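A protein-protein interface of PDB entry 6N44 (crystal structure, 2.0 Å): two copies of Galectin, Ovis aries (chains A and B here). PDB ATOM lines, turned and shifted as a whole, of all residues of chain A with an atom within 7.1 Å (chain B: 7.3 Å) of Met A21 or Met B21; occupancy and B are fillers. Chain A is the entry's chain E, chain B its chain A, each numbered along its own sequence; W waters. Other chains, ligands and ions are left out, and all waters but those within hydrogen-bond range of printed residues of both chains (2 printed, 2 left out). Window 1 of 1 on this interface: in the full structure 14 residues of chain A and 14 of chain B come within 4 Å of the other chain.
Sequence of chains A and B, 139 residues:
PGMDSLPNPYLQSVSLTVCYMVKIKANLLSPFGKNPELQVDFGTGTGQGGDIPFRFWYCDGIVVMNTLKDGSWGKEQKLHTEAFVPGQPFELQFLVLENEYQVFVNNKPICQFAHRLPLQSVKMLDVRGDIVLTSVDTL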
ATOM      1  N   LEU A  16      -7.591  14.168 -30.080  1.00  0.00           N
ATOM      2  CA  LEU A  16      -7.454  13.878 -28.661  1.00  0.00           C
ATOM      3  C   LEU A  16      -8.318  14.817 -27.822  1.00  0.00           C
ATOM      4  O   LEU A  16      -8.716  15.901 -28.257  1.00  0.00           O
ATOM      5  CB  LEU A  16      -5.995  14.011 -28.207  1.00  0.00           C
ATOM      6  CG  LEU A  16      -4.898  13.227 -28.932  1.00  0.00           C
ATOM      7  CD1 LEU A  16      -3.573  13.310 -28.132  1.00  0.00           C
ATOM      8  CD2 LEU A  16      -5.319  11.802 -29.097  1.00  0.00           C
ATOM      9  N   THR A  17      -8.593  14.389 -26.594  1.00  0.00           N
ATOM     10  CA  THR A  17      -9.254  15.237 -25.609  1.00  0.00           C
ATOM     11  C   THR A  17      -8.517  15.077 -24.286  1.00  0.00           C
ATOM     12  O   THR A  17      -7.488  14.402 -24.200  1.00  0.00           O
ATOM     13  CB  THR A  17     -10.736  14.878 -25.425  1.00  0.00           C
ATOM     14  OG1 THR A  17     -10.824  13.615 -24.757  1.00  0.00           O
ATOM     15  CG2 THR A  17     -11.495  14.814 -26.764  1.00  0.00           C
ATOM     16  N   CYS A  19      -9.661  13.418 -21.819  1.00  0.00           N
ATOM     17  CA  CYS A  19     -10.006  12.109 -21.280  1.00  0.00           C
ATOM     18  C   CYS A  19     -10.151  11.204 -22.502  1.00  0.00           C
ATOM     19  O   CYS A  19     -11.248  11.023 -23.030  1.00  0.00           O
ATOM     20  CB  CYS A  19     -11.279  12.139 -20.446  1.00  0.00           C
ATOM     21  SG  CYS A  19     -11.605  10.567 -19.595  1.00  0.00           S
ATOM     22  N   TYR A  20      -9.024  10.661 -22.948  1.00  0.00           N
ATOM     23  CA  TYR A  20      -8.940   9.951 -24.213  1.00  0.00           C
ATOM     24  C   TYR A  20      -8.007   8.774 -24.015  1.00  0.00           C
ATOM     25  O   TYR A  20      -6.989   8.892 -23.327  1.00  0.00           O
ATOM     26  CB  TYR A  20      -8.411  10.876 -25.319  1.00  0.00           C
ATOM     27  CG  TYR A  20      -8.430  10.326 -26.726  1.00  0.00           C
ATOM     28  CD1 TYR A  20      -9.470  10.640 -27.606  1.00  0.00           C
ATOM     29  CD2 TYR A  20      -7.390   9.526 -27.191  1.00  0.00           C
ATOM     30  CE1 TYR A  20      -9.473  10.165 -28.898  1.00  0.00           C
ATOM     31  CE2 TYR A  20      -7.376   9.044 -28.475  1.00  0.00           C
ATOM     32  CZ  TYR A  20      -8.419   9.364 -29.331  1.00  0.00           C
ATOM     33  OH  TYR A  20      -8.401   8.885 -30.623  1.00  0.00           O
ATOM     34  N   MET A  21      -8.356   7.642 -24.600  1.00  0.00           N
ATOM     35  CA  MET A  21      -7.579   6.439 -24.386  1.00  0.00           C
ATOM     36  C   MET A  21      -7.256   5.795 -25.722  1.00  0.00           C
ATOM     37  O   MET A  21      -8.091   5.757 -26.626  1.00  0.00           O
ATOM     38  CB  MET A  21      -8.315   5.441 -23.498  1.00  0.00           C
ATOM     39  CG  MET A  21      -7.439   4.257 -23.123  1.00  0.00           C
ATOM     40  SD  MET A  21      -8.351   2.800 -22.621  1.00  0.00           S
ATOM     41  CE  MET A  21      -9.050   3.388 -21.077  1.00  0.00           C
ATOM     42  N   VAL A  22      -6.029   5.307 -25.838  1.00  0.00           N
ATOM     43  CA  VAL A  22      -5.612   4.464 -26.947  1.00  0.00           C
ATOM     44  C   VAL A  22      -5.238   3.116 -26.352  1.00  0.00           C
ATOM     45  O   VAL A  22      -4.494   3.065 -25.367  1.00  0.00           O
ATOM     46  CB  VAL A  22      -4.415   5.072 -27.698  1.00  0.00           C
ATOM     47  CG1 VAL A  22      -3.964   4.147 -28.817  1.00  0.00           C
ATOM     48  CG2 VAL A  22      -4.752   6.490 -28.198  1.00  0.00           C
ATOM     49  N   LYS A  23      -5.749   2.030 -26.933  1.00  0.00           N
ATOM     50  CA  LYS A  23      -5.381   0.693 -26.489  1.00  0.00           C
ATOM     51  C   LYS A  23      -4.861  -0.102 -27.673  1.00  0.00           C
ATOM     52  O   LYS A  23      -5.570  -0.281 -28.675  1.00  0.00           O
ATOM     53  CB  LYS A  23      -6.543  -0.055 -25.828  1.00  0.00           C
ATOM     54  CG  LYS A  23      -6.129  -1.465 -25.418  1.00  0.00           C
ATOM     55  CD  LYS A  23      -7.281  -2.283 -24.887  1.00  0.00           C
ATOM     56  CE  LYS A  23      -7.745  -1.772 -23.538  1.00  0.00           C
ATOM     57  NZ  LYS A  23      -8.928  -2.569 -23.085  1.00  0.00           N
ATOM     58  N   PHE A  42       2.279  10.124 -31.435  1.00  0.00           N
ATOM     59  CA  PHE A  42       1.152  11.050 -31.421  1.00  0.00           C
ATOM     60  C   PHE A  42       1.641  12.279 -32.185  1.00  0.00           C
ATOM     61  O   PHE A  42       2.259  13.188 -31.616  1.00  0.00           O
ATOM     62  CB  PHE A  42       0.700  11.359 -29.993  1.00  0.00           C
ATOM     63  CG  PHE A  42       0.056  10.176 -29.292  1.00  0.00           C
ATOM     64  CD1 PHE A  42       0.827   9.123 -28.826  1.00  0.00           C
ATOM     65  CD2 PHE A  42      -1.316  10.109 -29.132  1.00  0.00           C
ATOM     66  CE1 PHE A  42       0.230   8.013 -28.185  1.00  0.00           C
ATOM     67  CE2 PHE A  42      -1.921   9.010 -28.509  1.00  0.00           C
ATOM     68  CZ  PHE A  42      -1.162   7.970 -28.035  1.00  0.00           C
ATOM     69  N   GLU A  91      -0.575  -5.732 -24.031  1.00  0.00           N
ATOM     70  CA  GLU A  91      -1.560  -4.681 -24.187  1.00  0.00           C
ATOM     71  C   GLU A  91      -0.931  -3.377 -23.714  1.00  0.00           C
ATOM     72  O   GLU A  91      -0.462  -3.278 -22.573  1.00  0.00           O
ATOM     73  CB  GLU A  91      -2.832  -5.016 -23.415  1.00  0.00           C
ATOM     74  CG  GLU A  91      -3.908  -3.988 -23.592  1.00  0.00           C
ATOM     75  CD  GLU A  91      -5.052  -4.193 -22.618  1.00  0.00           C
ATOM     76  OE1 GLU A  91      -5.361  -3.237 -21.867  1.00  0.00           O
ATOM     77  OE2 GLU A  91      -5.618  -5.315 -22.602  1.00  0.00           O
ATOM     78  N   GLN A  93      -1.544   0.685 -23.269  1.00  0.00           N
ATOM     79  CA  GLN A  93      -2.520   1.762 -23.225  1.00  0.00           C
ATOM     80  C   GLN A  93      -1.839   3.111 -23.099  1.00  0.00           C
ATOM     81  O   GLN A  93      -0.872   3.258 -22.352  1.00  0.00           O
ATOM     82  CB  GLN A  93      -3.485   1.599 -22.063  1.00  0.00           C
ATOM     83  CG  GLN A  93      -4.461   0.478 -22.246  1.00  0.00           C
ATOM     84  CD  GLN A  93      -5.182   0.196 -20.966  1.00  0.00           C
ATOM     85  OE1 GLN A  93      -4.592  -0.348 -20.026  1.00  0.00           O
ATOM     86  NE2 GLN A  93      -6.450   0.614 -20.888  1.00  0.00           N
ATOM     87  N   PHE A  94      -2.378   4.101 -23.808  1.00  0.00           N
ATOM     88  CA  PHE A  94      -2.035   5.495 -23.578  1.00  0.00           C
ATOM     89  C   PHE A  94      -3.296   6.207 -23.124  1.00  0.00           C
ATOM     90  O   PHE A  94      -4.313   6.181 -23.826  1.00  0.00           O
ATOM     91  CB  PHE A  94      -1.462   6.152 -24.839  1.00  0.00           C
ATOM     92  CG  PHE A  94      -0.215   5.510 -25.333  1.00  0.00           C
ATOM     93  CD1 PHE A  94      -0.273   4.441 -26.222  1.00  0.00           C
ATOM     94  CD2 PHE A  94       1.022   5.964 -24.900  1.00  0.00           C
ATOM     95  CE1 PHE A  94       0.901   3.830 -26.676  1.00  0.00           C
ATOM     96  CE2 PHE A  94       2.193   5.352 -25.331  1.00  0.00           C
ATOM     97  CZ  PHE A  94       2.132   4.300 -26.228  1.00  0.00           C
ATOM     98  N   LEU A  95      -3.228   6.830 -21.951  1.00  0.00           N
ATOM     99  CA  LEU A  95      -4.300   7.671 -21.427  1.00  0.00           C
ATOM    100  C   LEU A  95      -3.892   9.127 -21.575  1.00  0.00           C
ATOM    101  O   LEU A  95      -2.861   9.535 -21.034  1.00  0.00           O
ATOM    102  CB  LEU A  95      -4.571   7.344 -19.954  1.00  0.00           C
ATOM    103  CG  LEU A  95      -5.962   7.602 -19.378  1.00  0.00           C
ATOM    104  CD1 LEU A  95      -7.085   6.890 -20.164  1.00  0.00           C
ATOM    105  CD2 LEU A  95      -5.959   7.190 -17.908  1.00  0.00           C
ATOM    106  N   VAL A  96      -4.706   9.912 -22.274  1.00  0.00           N
ATOM    107  CA  VAL A  96      -4.429  11.329 -22.499  1.00  0.00           C
ATOM    108  C   VAL A  96      -5.226  12.125 -21.481  1.00  0.00           C
ATOM    109  O   VAL A  96      -6.457  12.178 -21.561  1.00  0.00           O
ATOM    110  CB  VAL A  96      -4.791  11.776 -23.922  1.00  0.00           C
ATOM    111  CG1 VAL A  96      -4.430  13.256 -24.117  1.00  0.00           C
ATOM    112  CG2 VAL A  96      -4.128  10.883 -24.974  1.00  0.00           C
ATOM    113  N   ASP A 137      -7.476   0.513 -30.680  1.00  0.00           N
ATOM    114  CA  ASP A 137      -8.779   1.059 -30.350  1.00  0.00           C
ATOM    115  C   ASP A 137      -8.601   2.373 -29.626  1.00  0.00           C
ATOM    116  O   ASP A 137      -7.636   2.549 -28.879  1.00  0.00           O
ATOM    117  CB  ASP A 137      -9.590   0.116 -29.466  1.00  0.00           C
ATOM    118  CG  ASP A 137     -10.087  -1.077 -30.223  1.00  0.00           C
ATOM    119  OD1 ASP A 137     -10.997  -0.904 -31.061  1.00  0.00           O
ATOM    120  OD2 ASP A 137      -9.567  -2.179 -29.988  1.00  0.00           O
ATOM    121  N   THR A 138      -9.541   3.294 -29.852  1.00  0.00           N
ATOM    122  CA  THR A 138      -9.544   4.568 -29.152  1.00  0.00           C
ATOM    123  C   THR A 138     -10.952   4.867 -28.654  1.00  0.00           C
ATOM    124  O   THR A 138     -11.944   4.398 -29.223  1.00  0.00           O
ATOM    125  CB  THR A 138      -9.043   5.732 -30.042  1.00  0.00           C
ATOM    126  OG1 THR A 138      -9.971   5.960 -31.104  1.00  0.00           O
ATOM    127  CG2 THR A 138      -7.666   5.428 -30.654  1.00  0.00           C
ATOM    128  N   LEU A 139     -11.029   5.666 -27.589  1.00  0.00           N
ATOM    129  CA  LEU A 139     -12.308   6.123 -27.030  1.00  0.00           C
ATOM    130  C   LEU A 139     -12.105   7.468 -26.335  1.00  0.00           C
ATOM    131  O   LEU A 139     -11.111   7.631 -25.608  1.00  0.00           O
ATOM    132  CB  LEU A 139     -12.881   5.098 -26.033  1.00  0.00           C
ATOM    133  CG  LEU A 139     -14.290   5.398 -25.511  1.00  0.00           C
ATOM    134  CD1 LEU A 139     -15.264   5.491 -26.686  1.00  0.00           C
ATOM    135  CD2 LEU A 139     -14.778   4.354 -24.514  1.00  0.00           C
ATOM    136  N   LEU B  16     -13.460  -4.037 -14.497  1.00  0.00           N
ATOM    137  CA  LEU B  16     -12.720  -2.795 -14.494  1.00  0.00           C
ATOM    138  C   LEU B  16     -11.227  -3.073 -14.403  1.00  0.00           C
ATOM    139  O   LEU B  16     -10.784  -4.108 -13.905  1.00  0.00           O
ATOM    140  CB  LEU B  16     -13.137  -1.907 -13.321  1.00  0.00           C
ATOM    141  CG  LEU B  16     -14.615  -1.507 -13.239  1.00  0.00           C
ATOM    142  CD1 LEU B  16     -14.822  -0.500 -12.115  1.00  0.00           C
ATOM    143  CD2 LEU B  16     -15.108  -0.941 -14.555  1.00  0.00           C
ATOM    144  N   THR B  17     -10.450  -2.121 -14.889  1.00  0.00           N
ATOM    145  CA  THR B  17      -9.024  -2.166 -14.626  1.00  0.00           C
ATOM    146  C   THR B  17      -8.597  -0.815 -14.087  1.00  0.00           C
ATOM    147  O   THR B  17      -9.423   0.079 -13.874  1.00  0.00           O
ATOM    148  CB  THR B  17      -8.229  -2.488 -15.891  1.00  0.00           C
ATOM    149  OG1 THR B  17      -8.367  -1.394 -16.812  1.00  0.00           O
ATOM    150  CG2 THR B  17      -8.704  -3.792 -16.538  1.00  0.00           C
ATOM    151  N   VAL B  18      -7.284  -0.667 -13.925  1.00  0.00           N
ATOM    152  CA  VAL B  18      -6.639   0.550 -13.453  1.00  0.00           C
ATOM    153  C   VAL B  18      -6.535   1.619 -14.532  1.00  0.00           C
ATOM    154  O   VAL B  18      -6.111   2.752 -14.250  1.00  0.00           O
ATOM    155  CB  VAL B  18      -5.332  -0.027 -12.872  1.00  0.00           C
ATOM    156  CG1 VAL B  18      -4.095   0.476 -13.587  1.00  0.00           C
ATOM    157  CG2 VAL B  18      -5.302   0.104 -11.376  1.00  0.00           C
ATOM    158  N   CYS B  19      -6.927   1.295 -15.770  1.00  0.00           N
ATOM    159  CA  CYS B  19      -6.991   2.275 -16.856  1.00  0.00           C
ATOM    160  C   CYS B  19      -8.180   1.872 -17.726  1.00  0.00           C
ATOM    161  O   CYS B  19      -8.025   1.106 -18.677  1.00  0.00           O
ATOM    162  CB  CYS B  19      -5.706   2.326 -17.674  1.00  0.00           C
ATOM    163  SG  CYS B  19      -5.801   3.585 -18.976  1.00  0.00           S
ATOM    164  N   TYR B  20      -9.356   2.395 -17.376  1.00  0.00           N
ATOM    165  CA  TYR B  20     -10.630   1.937 -17.925  1.00  0.00           C
ATOM    166  C   TYR B  20     -11.561   3.125 -18.122  1.00  0.00           C
ATOM    167  O   TYR B  20     -11.668   3.982 -17.243  1.00  0.00           O
ATOM    168  CB  TYR B  20     -11.274   0.915 -16.979  1.00  0.00           C
ATOM    169  CG  TYR B  20     -12.462   0.178 -17.541  1.00  0.00           C
ATOM    170  CD1 TYR B  20     -12.311  -1.093 -18.105  1.00  0.00           C
ATOM    171  CD2 TYR B  20     -13.730   0.734 -17.499  1.00  0.00           C
ATOM    172  CE1 TYR B  20     -13.395  -1.785 -18.611  1.00  0.00           C
ATOM    173  CE2 TYR B  20     -14.836   0.053 -18.004  1.00  0.00           C
ATOM    174  CZ  TYR B  20     -14.659  -1.198 -18.561  1.00  0.00           C
ATOM    175  OH  TYR B  20     -15.747  -1.879 -19.036  1.00  0.00           O
ATOM    176  N   MET B  21     -12.248   3.168 -19.261  1.00  0.00           N
ATOM    177  CA  MET B  21     -13.108   4.294 -19.595  1.00  0.00           C
ATOM    178  C   MET B  21     -14.510   3.821 -19.936  1.00  0.00           C
ATOM    179  O   MET B  21     -14.678   2.845 -20.675  1.00  0.00           O
ATOM    180  CB  MET B  21     -12.574   5.098 -20.762  1.00  0.00           C
ATOM    181  CG  MET B  21     -13.454   6.315 -21.064  1.00  0.00           C
ATOM    182  SD  MET B  21     -12.842   7.208 -22.490  1.00  0.00           S
ATOM    183  CE  MET B  21     -11.165   7.495 -21.955  1.00  0.00           C
ATOM    184  N   VAL B  22     -15.501   4.518 -19.380  1.00  0.00           N
ATOM    185  CA  VAL B  22     -16.904   4.413 -19.762  1.00  0.00           C
ATOM    186  C   VAL B  22     -17.303   5.741 -20.384  1.00  0.00           C
ATOM    187  O   VAL B  22     -17.055   6.802 -19.795  1.00  0.00           O
ATOM    188  CB  VAL B  22     -17.807   4.117 -18.550  1.00  0.00           C
ATOM    189  CG1 VAL B  22     -19.291   4.040 -18.993  1.00  0.00           C
ATOM    190  CG2 VAL B  22     -17.362   2.844 -17.815  1.00  0.00           C
ATOM    191  N   LYS B  23     -17.922   5.693 -21.562  1.00  0.00           N
ATOM    192  CA  LYS B  23     -18.423   6.894 -22.218  1.00  0.00           C
ATOM    193  C   LYS B  23     -19.903   6.717 -22.514  1.00  0.00           C
ATOM    194  O   LYS B  23     -20.277   5.844 -23.303  1.00  0.00           O
ATOM    195  CB  LYS B  23     -17.676   7.197 -23.513  1.00  0.00           C
ATOM    196  CG  LYS B  23     -18.143   8.518 -24.122  1.00  0.00           C
ATOM    197  CD  LYS B  23     -17.537   8.799 -25.473  1.00  0.00           C
ATOM    198  CE  LYS B  23     -16.017   8.777 -25.418  1.00  0.00           C
ATOM    199  NZ  LYS B  23     -15.441   9.345 -26.690  1.00  0.00           N
ATOM    200  N   PHE B  42     -21.831   1.496 -10.759  1.00  0.00           N
ATOM    201  CA  PHE B  42     -20.780   0.492 -10.883  1.00  0.00           C
ATOM    202  C   PHE B  42     -21.021  -0.481  -9.736  1.00  0.00           C
ATOM    203  O   PHE B  42     -20.590  -0.251  -8.602  1.00  0.00           O
ATOM    204  CB  PHE B  42     -19.400   1.133 -10.814  1.00  0.00           C
ATOM    205  CG  PHE B  42     -19.072   2.032 -11.992  1.00  0.00           C
ATOM    206  CD1 PHE B  42     -19.623   3.298 -12.102  1.00  0.00           C
ATOM    207  CD2 PHE B  42     -18.200   1.603 -12.985  1.00  0.00           C
ATOM    208  CE1 PHE B  42     -19.298   4.126 -13.186  1.00  0.00           C
ATOM    209  CE2 PHE B  42     -17.888   2.417 -14.068  1.00  0.00           C
ATOM    210  CZ  PHE B  42     -18.431   3.680 -14.164  1.00  0.00           C
ATOM    211  N   GLU B  91     -22.227  14.264 -23.032  1.00  0.00           N
ATOM    212  CA  GLU B  91     -21.309  13.142 -22.966  1.00  0.00           C
ATOM    213  C   GLU B  91     -20.761  13.034 -21.551  1.00  0.00           C
ATOM    214  O   GLU B  91     -20.053  13.933 -21.084  1.00  0.00           O
ATOM    215  CB  GLU B  91     -20.169  13.314 -23.965  1.00  0.00           C
ATOM    216  CG  GLU B  91     -19.148  12.225 -23.861  1.00  0.00           C
ATOM    217  CD  GLU B  91     -18.015  12.430 -24.848  1.00  0.00           C
ATOM    218  OE1 GLU B  91     -16.846  12.388 -24.412  1.00  0.00           O
ATOM    219  OE2 GLU B  91     -18.308  12.658 -26.046  1.00  0.00           O
ATOM    220  N   LEU B  92     -21.078  11.936 -20.880  1.00  0.00           N
ATOM    221  CA  LEU B  92     -20.634  11.672 -19.523  1.00  0.00           C
ATOM    222  C   LEU B  92     -19.572  10.578 -19.567  1.00  0.00           C
ATOM    223  O   LEU B  92     -19.824   9.482 -20.091  1.00  0.00           O
ATOM    224  CB  LEU B  92     -21.819  11.270 -18.647  1.00  0.00           C
ATOM    225  CG  LEU B  92     -21.546  10.648 -17.279  1.00  0.00           C
ATOM    226  CD1 LEU B  92     -20.853  11.637 -16.324  1.00  0.00           C
ATOM    227  CD2 LEU B  92     -22.858  10.156 -16.694  1.00  0.00           C
ATOM    228  N   GLN B  93     -18.389  10.874 -19.026  1.00  0.00           N
ATOM    229  CA  GLN B  93     -17.276   9.927 -19.006  1.00  0.00           C
ATOM    230  C   GLN B  93     -16.879   9.582 -17.581  1.00  0.00           C
ATOM    231  O   GLN B  93     -16.702  10.481 -16.748  1.00  0.00           O
ATOM    232  CB  GLN B  93     -16.045  10.491 -19.716  1.00  0.00           C
ATOM    233  CG  GLN B  93     -16.116  10.517 -21.220  1.00  0.00           C
ATOM    234  CD  GLN B  93     -14.905  11.223 -21.788  1.00  0.00           C
ATOM    235  OE1 GLN B  93     -14.768  12.448 -21.647  1.00  0.00           O
ATOM    236  NE2 GLN B  93     -13.984  10.450 -22.379  1.00  0.00           N
ATOM    237  N   PHE B  94     -16.671   8.289 -17.325  1.00  0.00           N
ATOM    238  CA  PHE B  94     -16.041   7.822 -16.100  1.00  0.00           C
ATOM    239  C   PHE B  94     -14.704   7.204 -16.454  1.00  0.00           C
ATOM    240  O   PHE B  94     -14.624   6.319 -17.312  1.00  0.00           O
ATOM    241  CB  PHE B  94     -16.906   6.789 -15.353  1.00  0.00           C
ATOM    242  CG  PHE B  94     -18.229   7.323 -14.893  1.00  0.00           C
ATOM    243  CD1 PHE B  94     -19.337   7.273 -15.728  1.00  0.00           C
ATOM    244  CD2 PHE B  94     -18.365   7.876 -13.634  1.00  0.00           C
ATOM    245  CE1 PHE B  94     -20.579   7.762 -15.315  1.00  0.00           C
ATOM    246  CE2 PHE B  94     -19.600   8.373 -13.203  1.00  0.00           C
ATOM    247  CZ  PHE B  94     -20.715   8.312 -14.049  1.00  0.00           C
ATOM    248  N   LEU B  95     -13.665   7.666 -15.787  1.00  0.00           N
ATOM    249  CA  LEU B  95     -12.318   7.144 -15.936  1.00  0.00           C
ATOM    250  C   LEU B  95     -11.959   6.404 -14.661  1.00  0.00           C
ATOM    251  O   LEU B  95     -11.900   7.019 -13.594  1.00  0.00           O
ATOM    252  CB  LEU B  95     -11.342   8.291 -16.198  1.00  0.00           C
ATOM    253  CG  LEU B  95      -9.905   7.906 -16.511  1.00  0.00           C
ATOM    254  CD1 LEU B  95      -9.842   6.953 -17.706  1.00  0.00           C
ATOM    255  CD2 LEU B  95      -9.111   9.198 -16.761  1.00  0.00           C
ATOM    256  N   VAL B  96     -11.741   5.093 -14.762  1.00  0.00           N
ATOM    257  CA  VAL B  96     -11.355   4.294 -13.604  1.00  0.00           C
ATOM    258  C   VAL B  96      -9.828   4.244 -13.537  1.00  0.00           C
ATOM    259  O   VAL B  96      -9.163   3.766 -14.463  1.00  0.00           O
ATOM    260  CB  VAL B  96     -11.963   2.882 -13.658  1.00  0.00           C
ATOM    261  CG1 VAL B  96     -11.721   2.160 -12.352  1.00  0.00           C
ATOM    262  CG2 VAL B  96     -13.462   2.954 -13.956  1.00  0.00           C
ATOM    263  N   ASP B 137     -20.130   3.152 -24.282  1.00  0.00           N
ATOM    264  CA  ASP B 137     -18.943   2.497 -24.783  1.00  0.00           C
ATOM    265  C   ASP B 137     -17.949   2.342 -23.651  1.00  0.00           C
ATOM    266  O   ASP B 137     -17.877   3.186 -22.751  1.00  0.00           O
ATOM    267  CB  ASP B 137     -18.320   3.290 -25.930  1.00  0.00           C
ATOM    268  CG  ASP B 137     -19.183   3.284 -27.157  1.00  0.00           C
ATOM    269  OD1 ASP B 137     -19.253   2.221 -27.800  1.00  0.00           O
ATOM    270  OD2 ASP B 137     -19.806   4.327 -27.475  1.00  0.00           O
ATOM    271  N   THR B 138     -17.176   1.258 -23.700  1.00  0.00           N
ATOM    272  CA  THR B 138     -16.150   1.020 -22.699  1.00  0.00           C
ATOM    273  C   THR B 138     -14.850   0.605 -23.380  1.00  0.00           C
ATOM    274  O   THR B 138     -14.846  -0.008 -24.452  1.00  0.00           O
ATOM    275  CB  THR B 138     -16.576  -0.052 -21.679  1.00  0.00           C
ATOM    276  OG1 THR B 138     -16.671  -1.320 -22.333  1.00  0.00           O
ATOM    277  CG2 THR B 138     -17.934   0.286 -21.023  1.00  0.00           C
ATOM    278  N   LEU B 139     -13.748   0.962 -22.738  1.00  0.00           N
ATOM    279  CA  LEU B 139     -12.410   0.600 -23.180  1.00  0.00           C
ATOM    280  C   LEU B 139     -11.456   0.661 -21.974  1.00  0.00           C
ATOM    281  O   LEU B 139     -10.655  -0.262 -21.786  1.00  0.00           O
ATOM    282  CB  LEU B 139     -11.923   1.527 -24.299  1.00  0.00           C
ATOM    283  CG  LEU B 139     -10.596   1.121 -24.919  1.00  0.00           C
ATOM    284  CD1 LEU B 139     -10.749  -0.191 -25.698  1.00  0.00           C
ATOM    285  CD2 LEU B 139     -10.054   2.247 -25.803  1.00  0.00           C
HETATM  286  O   HOH W   1     -12.570  10.745 -25.440  1.00  0.00           O
HETATM  287  O   HOH W   2      -6.099  -1.677 -18.237  1.00  0.00           O
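Water W2 lies within hydrogen-bond range of OE1 of Gln A93 (2.7 Å), OG1 of Thr B17 (2.7 Å) and O of Cys B19 (3.4 Å). Water W1 lies within hydrogen-bond range of the backbone carbonyl oxygen (O) of Cys A19 (2.8 Å), the side-chain amide nitrogen (NE2) of Gln B93 (3.4 Å), the side-chain hydroxyl (OG1) of Thr A17 (3.4 Å), the side-chain amino group (NZ) of Lys B23 (3.4 Å) and the backbone carbonyl oxygen (O) of Leu A139 (3.4 Å).
Cys A19 touches Gln B93, and with the chains exchanged Gln A93 touches Cys B19. Tyr A20 touches Met B21, and with the chains exchanged Met A21 touches Tyr B20. Asp A137 touches Leu B139, and with the chains exchanged Leu A139 touches Asp B137. Thr A138 touches Leu B139, and with the chains exchanged Leu A139 touches Thr B138. Of the 18 pairs that touch across the chains among the printed residues, 17 have their exchanged pair printed and touching as well.
The backbone carbonyl oxygen (O) of Cys A19 sits at hydrogen-bond distance from the side-chain amide nitrogen (NE2) of Gln B93 (2.9 Å). The backbone carbonyl oxygen (O) of Cys B19 is in hydrogen-bond range of the side-chain amide nitrogen (NE2) of Gln A93. The backbone carbonyl oxygen of Leu A139 sits close to the side-chain sulfur of Met B21. The backbone carbonyl oxygen (O) of Leu B139 lies within hydrogen-bond range of the side-chain amino group (NZ) of Lys A23 (3.2 Å).
The backbone carbonyl oxygen (O) of Val A96 lies within hydrogen-bond range of the backbone NH (N) of Cys A19 (3.4 Å). O of Cys A19 is in hydrogen-bond range of OG1 of Thr A17 (3.1 Å). O of Met B21 sits at hydrogen-bond distance from N of Leu B139. SD of Met B21 lies within hydrogen-bond range of NE2 of Gln B93, 3.4 Å away. OH of Tyr B20 lies close to OG1 of Thr B138 (3.5 Å). The backbone NH of Val A96 is in hydrogen-bond range of the backbone carbonyl oxygen of Tyr A20 (2.7 Å).
Met B21 touches Tyr A20 (CE to N, 3.9 Å). Met A21 touches Cys B19. Met A21 touches Met B21 (CE to N, 3.7 Å). SD of Met A21 touches CG of Leu B139, 3.6 Å away. Asp A137 touches Leu B139. Leu B139 touches Thr A138. Lys B23 touches Leu A139. Leu A139 touches Asp B137. CD2 of Leu A139 touches C of Thr B138 (3.9 Å). CD2 of Leu A139 touches N of Leu B139, at 3.96 Å.
Hydrophobic or aromatic side chains of chain B within 4 Å of the printed part of chain A: Met B21, Leu B95 and Leu B139. Printed residues of chain A that touch a printed residue of chain B: Cys A19, Tyr A20, Met A21, Lys A23, Gln A93, Leu A95, Asp A137, Thr A138 and Leu A139. Among the printed residues, 18 pairs touch across the chains. Among the printed residues, no Asp or Glu carboxylate lies within 4 Å of a Lys or Arg side-chain nitrogen of the other chain.
Met A21 touches just these residues of chain B: Cys B19, Tyr B20, Met B21 and Leu B139. Of the printed residues of chain B, Lys A23 touches Leu B139 (3.2 Å). Printed residues of chain B within 4 Å of Leu A139: Met B21 (3.6 Å), Lys B23 (3.6 Å), Asp B137 (3.8 Å), Thr B138 (3.9 Å) and Leu B139 (3.96 Å). Val B18 touches none of the printed residues of chain A. Leu B92 touches none of the printed residues of chain A. Of the printed residues of chain A, Thr B138 touches Leu A139. Of the printed residues of chain A, Leu B139 touches Met A21 (3.6 Å), Lys A23 (3.2 Å), Asp A137 (3.9 Å), Thr A138 (3.97 Å) and Leu A139 (3.96 Å).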
